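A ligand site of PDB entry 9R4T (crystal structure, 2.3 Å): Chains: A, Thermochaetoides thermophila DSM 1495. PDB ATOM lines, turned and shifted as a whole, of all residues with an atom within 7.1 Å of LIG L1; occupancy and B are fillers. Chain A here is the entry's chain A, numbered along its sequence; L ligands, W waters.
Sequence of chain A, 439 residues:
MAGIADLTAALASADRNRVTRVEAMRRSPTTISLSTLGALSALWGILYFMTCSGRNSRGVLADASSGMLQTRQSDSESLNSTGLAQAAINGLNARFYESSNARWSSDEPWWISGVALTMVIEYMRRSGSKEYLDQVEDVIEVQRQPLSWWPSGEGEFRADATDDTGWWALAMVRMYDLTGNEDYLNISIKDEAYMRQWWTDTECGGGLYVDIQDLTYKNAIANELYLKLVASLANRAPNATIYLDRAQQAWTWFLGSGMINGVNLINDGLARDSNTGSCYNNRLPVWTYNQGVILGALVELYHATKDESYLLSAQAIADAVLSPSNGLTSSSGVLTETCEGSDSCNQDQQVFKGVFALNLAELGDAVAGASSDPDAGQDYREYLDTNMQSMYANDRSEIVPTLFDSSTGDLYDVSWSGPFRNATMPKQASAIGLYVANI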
ATOM      1  N   ASP A 163      -8.966  26.500  25.412  1.00  0.00           N
ATOM      2  CA  ASP A 163      -7.520  26.447  25.460  1.00  0.00           C
ATOM      3  C   ASP A 163      -6.885  27.383  24.431  1.00  0.00           C
ATOM      4  O   ASP A 163      -5.827  27.968  24.701  1.00  0.00           O
ATOM      5  CB  ASP A 163      -7.010  25.017  25.275  1.00  0.00           C
ATOM      6  CG  ASP A 163      -7.507  24.374  23.988  1.00  0.00           C
ATOM      7  OD1 ASP A 163      -8.349  24.971  23.296  1.00  0.00           O
ATOM      8  OD2 ASP A 163      -7.035  23.264  23.674  1.00  0.00           O
ATOM      9  N   VAL A 210     -13.247  22.049  26.824  1.00  0.00           N
ATOM     10  CA  VAL A 210     -12.370  22.614  25.795  1.00  0.00           C
ATOM     11  C   VAL A 210     -13.154  22.981  24.544  1.00  0.00           C
ATOM     12  O   VAL A 210     -12.889  24.012  23.916  1.00  0.00           O
ATOM     13  CB  VAL A 210     -11.213  21.636  25.483  1.00  0.00           C
ATOM     14  CG1 VAL A 210     -11.751  20.295  24.993  1.00  0.00           C
ATOM     15  CG2 VAL A 210     -10.258  22.247  24.465  1.00  0.00           C
ATOM     16  N   TYR A 217     -15.866  17.398  26.263  1.00  0.00           N
ATOM     17  CA  TYR A 217     -14.525  16.997  26.680  1.00  0.00           C
ATOM     18  C   TYR A 217     -13.958  18.027  27.661  1.00  0.00           C
ATOM     19  O   TYR A 217     -13.744  19.182  27.295  1.00  0.00           O
ATOM     20  CB  TYR A 217     -13.604  16.859  25.462  1.00  0.00           C
ATOM     21  CG  TYR A 217     -12.303  16.164  25.744  1.00  0.00           C
ATOM     22  CD1 TYR A 217     -12.170  15.277  26.809  1.00  0.00           C
ATOM     23  CD2 TYR A 217     -11.192  16.372  24.931  1.00  0.00           C
ATOM     24  CE1 TYR A 217     -10.975  14.640  27.067  1.00  0.00           C
ATOM     25  CE2 TYR A 217      -9.992  15.736  25.181  1.00  0.00           C
ATOM     26  CZ  TYR A 217      -9.884  14.864  26.242  1.00  0.00           C
ATOM     27  OH  TYR A 217      -8.690  14.228  26.501  1.00  0.00           O
ATOM     28  N   ASN A 219     -10.550  18.340  29.268  1.00  0.00           N
ATOM     29  CA  ASN A 219      -9.211  17.789  29.116  1.00  0.00           C
ATOM     30  C   ASN A 219      -8.237  18.476  30.065  1.00  0.00           C
ATOM     31  O   ASN A 219      -8.600  19.397  30.804  1.00  0.00           O
ATOM     32  CB  ASN A 219      -8.753  17.899  27.654  1.00  0.00           C
ATOM     33  CG  ASN A 219      -8.658  19.338  27.170  1.00  0.00           C
ATOM     34  OD1 ASN A 219      -8.892  20.276  27.924  1.00  0.00           O
ATOM     35  ND2 ASN A 219      -8.311  19.504  25.899  1.00  0.00           N
ATOM     36  N   ALA A 220      -6.991  18.019  30.035  1.00  0.00           N
ATOM     37  CA  ALA A 220      -5.990  18.526  30.973  1.00  0.00           C
ATOM     38  C   ALA A 220      -5.497  19.917  30.576  1.00  0.00           C
ATOM     39  O   ALA A 220      -5.308  20.782  31.442  1.00  0.00           O
ATOM     40  CB  ALA A 220      -4.827  17.554  31.078  1.00  0.00           C
ATOM     41  N   ILE A 221      -5.304  20.153  29.277  1.00  0.00           N
ATOM     42  CA  ILE A 221      -4.602  21.367  28.856  1.00  0.00           C
ATOM     43  C   ILE A 221      -5.463  22.599  29.079  1.00  0.00           C
ATOM     44  O   ILE A 221      -4.969  23.641  29.524  1.00  0.00           O
ATOM     45  CB  ILE A 221      -4.127  21.234  27.385  1.00  0.00           C
ATOM     46  CG1 ILE A 221      -3.216  22.412  27.025  1.00  0.00           C
ATOM     47  CG2 ILE A 221      -5.297  21.101  26.420  1.00  0.00           C
ATOM     48  CD1 ILE A 221      -2.058  22.604  27.985  1.00  0.00           C
ATOM     49  N   ALA A 222      -6.765  22.516  28.775  1.00  0.00           N
ATOM     50  CA  ALA A 222      -7.628  23.673  28.972  1.00  0.00           C
ATOM     51  C   ALA A 222      -7.758  24.027  30.448  1.00  0.00           C
ATOM     52  O   ALA A 222      -7.835  25.207  30.803  1.00  0.00           O
ATOM     53  CB  ALA A 222      -9.009  23.417  28.366  1.00  0.00           C
ATOM     54  N   ASP A 268      -4.355  12.798  29.197  1.00  0.00           N
ATOM     55  CA  ASP A 268      -4.866  13.876  28.361  1.00  0.00           C
ATOM     56  C   ASP A 268      -6.129  14.518  28.938  1.00  0.00           C
ATOM     57  O   ASP A 268      -6.297  15.736  28.863  1.00  0.00           O
ATOM     58  CB  ASP A 268      -5.132  13.369  26.943  1.00  0.00           C
ATOM     59  CG  ASP A 268      -5.229  14.493  25.940  1.00  0.00           C
ATOM     60  OD1 ASP A 268      -4.217  15.194  25.750  1.00  0.00           O
ATOM     61  OD2 ASP A 268      -6.314  14.681  25.330  1.00  0.00           O
ATOM     62  N   GLY A 269      -7.021  13.719  29.515  1.00  0.00           N
ATOM     63  CA  GLY A 269      -8.260  14.286  30.000  1.00  0.00           C
ATOM     64  C   GLY A 269      -9.117  13.272  30.729  1.00  0.00           C
ATOM     65  O   GLY A 269      -8.630  12.240  31.197  1.00  0.00           O
ATOM     66  N   LEU A 284      -5.544   8.480  27.973  1.00  0.00           N
ATOM     67  CA  LEU A 284      -4.989   8.932  26.712  1.00  0.00           C
ATOM     68  C   LEU A 284      -3.542   9.392  26.912  1.00  0.00           C
ATOM     69  O   LEU A 284      -3.113   9.600  28.047  1.00  0.00           O
ATOM     70  CB  LEU A 284      -5.859  10.054  26.134  1.00  0.00           C
ATOM     71  CG  LEU A 284      -7.117   9.576  25.408  1.00  0.00           C
ATOM     72  CD1 LEU A 284      -7.732  10.709  24.606  1.00  0.00           C
ATOM     73  CD2 LEU A 284      -6.812   8.385  24.515  1.00  0.00           C
ATOM     74  N   PRO A 285      -2.754   9.524  25.811  1.00  0.00           N
ATOM     75  CA  PRO A 285      -1.303   9.724  25.948  1.00  0.00           C
ATOM     76  C   PRO A 285      -0.856  10.810  26.909  1.00  0.00           C
ATOM     77  O   PRO A 285      -1.592  11.765  27.195  1.00  0.00           O
ATOM     78  CB  PRO A 285      -0.874  10.066  24.522  1.00  0.00           C
ATOM     79  CG  PRO A 285      -1.820   9.302  23.678  1.00  0.00           C
ATOM     80  CD  PRO A 285      -3.138   9.332  24.404  1.00  0.00           C
ATOM     81  N   TRP A 287       1.262  13.789  27.199  1.00  0.00           N
ATOM     82  CA  TRP A 287       1.916  14.787  26.377  1.00  0.00           C
ATOM     83  C   TRP A 287       2.759  15.718  27.248  1.00  0.00           C
ATOM     84  O   TRP A 287       2.376  16.044  28.373  1.00  0.00           O
ATOM     85  CB  TRP A 287       0.882  15.594  25.582  1.00  0.00           C
ATOM     86  CG  TRP A 287       0.011  14.739  24.709  1.00  0.00           C
ATOM     87  CD1 TRP A 287      -1.316  14.478  24.893  1.00  0.00           C
ATOM     88  CD2 TRP A 287       0.391  14.049  23.515  1.00  0.00           C
ATOM     89  NE1 TRP A 287      -1.784  13.670  23.894  1.00  0.00           N
ATOM     90  CE2 TRP A 287      -0.761  13.387  23.029  1.00  0.00           C
ATOM     91  CE3 TRP A 287       1.589  13.925  22.812  1.00  0.00           C
ATOM     92  CZ2 TRP A 287      -0.735  12.611  21.873  1.00  0.00           C
ATOM     93  CZ3 TRP A 287       1.604  13.157  21.650  1.00  0.00           C
ATOM     94  CH2 TRP A 287       0.445  12.506  21.194  1.00  0.00           C
ATOM     95  N   TYR A 289       3.490  18.884  27.125  1.00  0.00           N
ATOM     96  CA  TYR A 289       2.969  20.185  27.507  1.00  0.00           C
ATOM     97  C   TYR A 289       1.895  20.097  28.575  1.00  0.00           C
ATOM     98  O   TYR A 289       1.536  21.128  29.157  1.00  0.00           O
ATOM     99  CB  TYR A 289       2.463  20.944  26.263  1.00  0.00           C
ATOM    100  CG  TYR A 289       1.083  20.572  25.746  1.00  0.00           C
ATOM    101  CD1 TYR A 289       0.593  19.267  25.814  1.00  0.00           C
ATOM    102  CD2 TYR A 289       0.262  21.540  25.168  1.00  0.00           C
ATOM    103  CE1 TYR A 289      -0.668  18.952  25.332  1.00  0.00           C
ATOM    104  CE2 TYR A 289      -0.986  21.228  24.682  1.00  0.00           C
ATOM    105  CZ  TYR A 289      -1.452  19.938  24.764  1.00  0.00           C
ATOM    106  OH  TYR A 289      -2.701  19.636  24.277  1.00  0.00           O
ATOM    107  N   ASN A 290       1.373  18.905  28.857  1.00  0.00           N
ATOM    108  CA  ASN A 290       0.480  18.694  29.989  1.00  0.00           C
ATOM    109  C   ASN A 290       1.225  18.404  31.278  1.00  0.00           C
ATOM    110  O   ASN A 290       0.589  18.319  32.341  1.00  0.00           O
ATOM    111  CB  ASN A 290      -0.498  17.550  29.692  1.00  0.00           C
ATOM    112  CG  ASN A 290      -1.726  18.015  28.927  1.00  0.00           C
ATOM    113  OD1 ASN A 290      -2.168  19.150  29.097  1.00  0.00           O
ATOM    114  ND2 ASN A 290      -2.272  17.145  28.089  1.00  0.00           N
ATOM    115  N   ASN A 346       2.001  15.443  14.944  1.00  0.00           N
ATOM    116  CA  ASN A 346       1.206  16.322  14.091  1.00  0.00           C
ATOM    117  C   ASN A 346       1.556  17.784  14.385  1.00  0.00           C
ATOM    118  O   ASN A 346       2.469  18.086  15.152  1.00  0.00           O
ATOM    119  CB  ASN A 346      -0.282  16.007  14.251  1.00  0.00           C
ATOM    120  CG  ASN A 346      -0.853  16.428  15.605  1.00  0.00           C
ATOM    121  OD1 ASN A 346      -0.167  17.029  16.435  1.00  0.00           O
ATOM    122  ND2 ASN A 346      -2.124  16.108  15.819  1.00  0.00           N
ATOM    123  N   ASP A 348       0.083  19.995  16.126  1.00  0.00           N
ATOM    124  CA  ASP A 348      -0.057  20.371  17.528  1.00  0.00           C
ATOM    125  C   ASP A 348       1.104  19.837  18.357  1.00  0.00           C
ATOM    126  O   ASP A 348       1.765  20.587  19.085  1.00  0.00           O
ATOM    127  CB  ASP A 348      -1.388  19.854  18.094  1.00  0.00           C
ATOM    128  CG  ASP A 348      -2.594  20.485  17.426  1.00  0.00           C
ATOM    129  OD1 ASP A 348      -2.518  21.686  17.076  1.00  0.00           O
ATOM    130  OD2 ASP A 348      -3.628  19.792  17.282  1.00  0.00           O
ATOM    131  N   GLN A 349       1.381  18.531  18.238  1.00  0.00           N
ATOM    132  CA  GLN A 349       2.386  17.886  19.078  1.00  0.00           C
ATOM    133  C   GLN A 349       3.802  18.361  18.790  1.00  0.00           C
ATOM    134  O   GLN A 349       4.701  18.122  19.604  1.00  0.00           O
ATOM    135  CB  GLN A 349       2.282  16.370  18.911  1.00  0.00           C
ATOM    136  CG  GLN A 349       0.931  15.793  19.291  1.00  0.00           C
ATOM    137  CD  GLN A 349       0.416  14.783  18.294  1.00  0.00           C
ATOM    138  OE1 GLN A 349       1.116  14.400  17.358  1.00  0.00           O
ATOM    139  NE2 GLN A 349      -0.829  14.342  18.473  1.00  0.00           N
ATOM    140  N   PHE A 352       4.912  20.859  21.658  1.00  0.00           N
ATOM    141  CA  PHE A 352       4.658  20.538  23.058  1.00  0.00           C
ATOM    142  C   PHE A 352       5.921  20.681  23.916  1.00  0.00           C
ATOM    143  O   PHE A 352       5.850  21.190  25.039  1.00  0.00           O
ATOM    144  CB  PHE A 352       4.100  19.123  23.188  1.00  0.00           C
ATOM    145  CG  PHE A 352       2.676  18.983  22.732  1.00  0.00           C
ATOM    146  CD1 PHE A 352       1.935  20.097  22.365  1.00  0.00           C
ATOM    147  CD2 PHE A 352       2.065  17.738  22.699  1.00  0.00           C
ATOM    148  CE1 PHE A 352       0.624  19.972  21.951  1.00  0.00           C
ATOM    149  CE2 PHE A 352       0.756  17.604  22.286  1.00  0.00           C
ATOM    150  CZ  PHE A 352       0.033  18.720  21.906  1.00  0.00           C
HETATM  151  C1  LIG L   1      -6.937  17.624  22.363  1.00  0.00           C
HETATM  152  C2  LIG L   1      -5.912  17.762  23.477  1.00  0.00           C
HETATM  153  C3  LIG L   1      -4.703  16.879  23.197  1.00  0.00           C
HETATM  154  C4  LIG L   1      -4.146  17.147  21.806  1.00  0.00           C
HETATM  155  C5  LIG L   1      -3.028  16.197  21.426  1.00  0.00           C
HETATM  156  C6  LIG L   1      -6.280  17.883  21.006  1.00  0.00           C
HETATM  157  O1  LIG L   1      -7.222  17.699  19.996  1.00  0.00           O
HETATM  158  O2  LIG L   1      -8.000  18.549  22.555  1.00  0.00           O
HETATM  159  O3  LIG L   1      -6.497  17.416  24.723  1.00  0.00           O
HETATM  160  O4  LIG L   1      -3.684  17.127  24.171  1.00  0.00           O
HETATM  161  O5  LIG L   1      -5.182  16.987  20.823  1.00  0.00           O
HETATM  162  O6  LIG L   1      -2.555  16.454  20.103  1.00  0.00           O
HETATM  163  C1  LG2 L   2     -13.840  12.393  25.636  1.00  0.00           C
HETATM  164  C2  LG2 L   2     -14.184  12.748  24.197  1.00  0.00           C
HETATM  165  C3  LG2 L   2     -12.944  13.254  23.465  1.00  0.00           C
HETATM  166  C4  LG2 L   2     -11.801  12.239  23.603  1.00  0.00           C
HETATM  167  C5  LG2 L   2     -10.508  12.725  22.993  1.00  0.00           C
HETATM  168  C6  LG2 L   2     -12.662  11.430  25.693  1.00  0.00           C
HETATM  169  O1  LG2 L   2     -12.317  11.188  27.020  1.00  0.00           O
HETATM  170  O2  LG2 L   2     -14.972  11.798  26.279  1.00  0.00           O
HETATM  171  O3  LG2 L   2     -15.196  13.745  24.167  1.00  0.00           O
HETATM  172  O4  LG2 L   2     -13.235  13.440  22.086  1.00  0.00           O
HETATM  173  O5  LG2 L   2     -11.548  11.985  24.994  1.00  0.00           O
HETATM  174  O6  LG2 L   2     -10.660  13.020  21.614  1.00  0.00           O
HETATM  175  O   HOH W   1      -4.053  16.991  17.888  1.00  0.00           O
HETATM  176  O   HOH W   2      -7.144  21.046  22.209  1.00  0.00           O
HETATM  177  O   HOH W   3      -5.138  17.908  27.220  1.00  0.00           O
HETATM  178  O   HOH W   4     -10.697  16.750  21.588  1.00  0.00           O
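An oxygen (O4) of LIG L1 lies within hydrogen-bond range of the side-chain carboxylate (OD1) of Asp 268, at 2.6 Å. OH of Tyr 289 sits at hydrogen-bond distance from O4 of LIG L1 (2.7 Å). An oxygen (O3) of LIG L1 is in hydrogen-bond range of the side-chain amide nitrogen of Asn 219 (3.0 Å). An oxygen (O6) of LIG L1 is in hydrogen-bond range of the side-chain amide nitrogen of Gln 349.
The side-chain carboxylate of Asp 268 lies close to the indole nitrogen of Trp 287, 3.4 Å away. The side-chain carboxylate of Asp 268 sits at hydrogen-bond distance from the side-chain hydroxyl of Tyr 217 (2.7 Å). O of Asp 268 sits at hydrogen-bond distance from N of Ala 220 (2.7 Å). OD1 of Asn 219 sits close to N of Ala 222 (3.2 Å). OE1 of Gln 349 lies within hydrogen-bond range of N of Asn 346. O of Tyr 217 is in hydrogen-bond range of N of Val 210. OH of Tyr 217 sits at hydrogen-bond distance from N of Gly 269, 3.5 Å away.
Tyr 217 touches LIG L1. Trp 287 touches LIG L1. CZ of Phe 352 touches O6 of LIG L1, at 3.9 Å. Hydrophobic or aromatic side chains within 4 Å of LIG L1: Tyr 217, Trp 287, Tyr 289 and Phe 352. Of the 18 residues printed, 7 come within 4 Å of LIG L1.
Water W2 bridges the side-chain carboxylate (OD2) of Asp 163 (2.7 Å) and an oxygen (O2) of LIG L1 (2.7 Å). Water W1 lies within hydrogen-bond range of O6 of LIG L1 (2.7 Å), OD2 of Asp 348 (2.9 Å) and ND2 of Asn 346 (3.0 Å).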
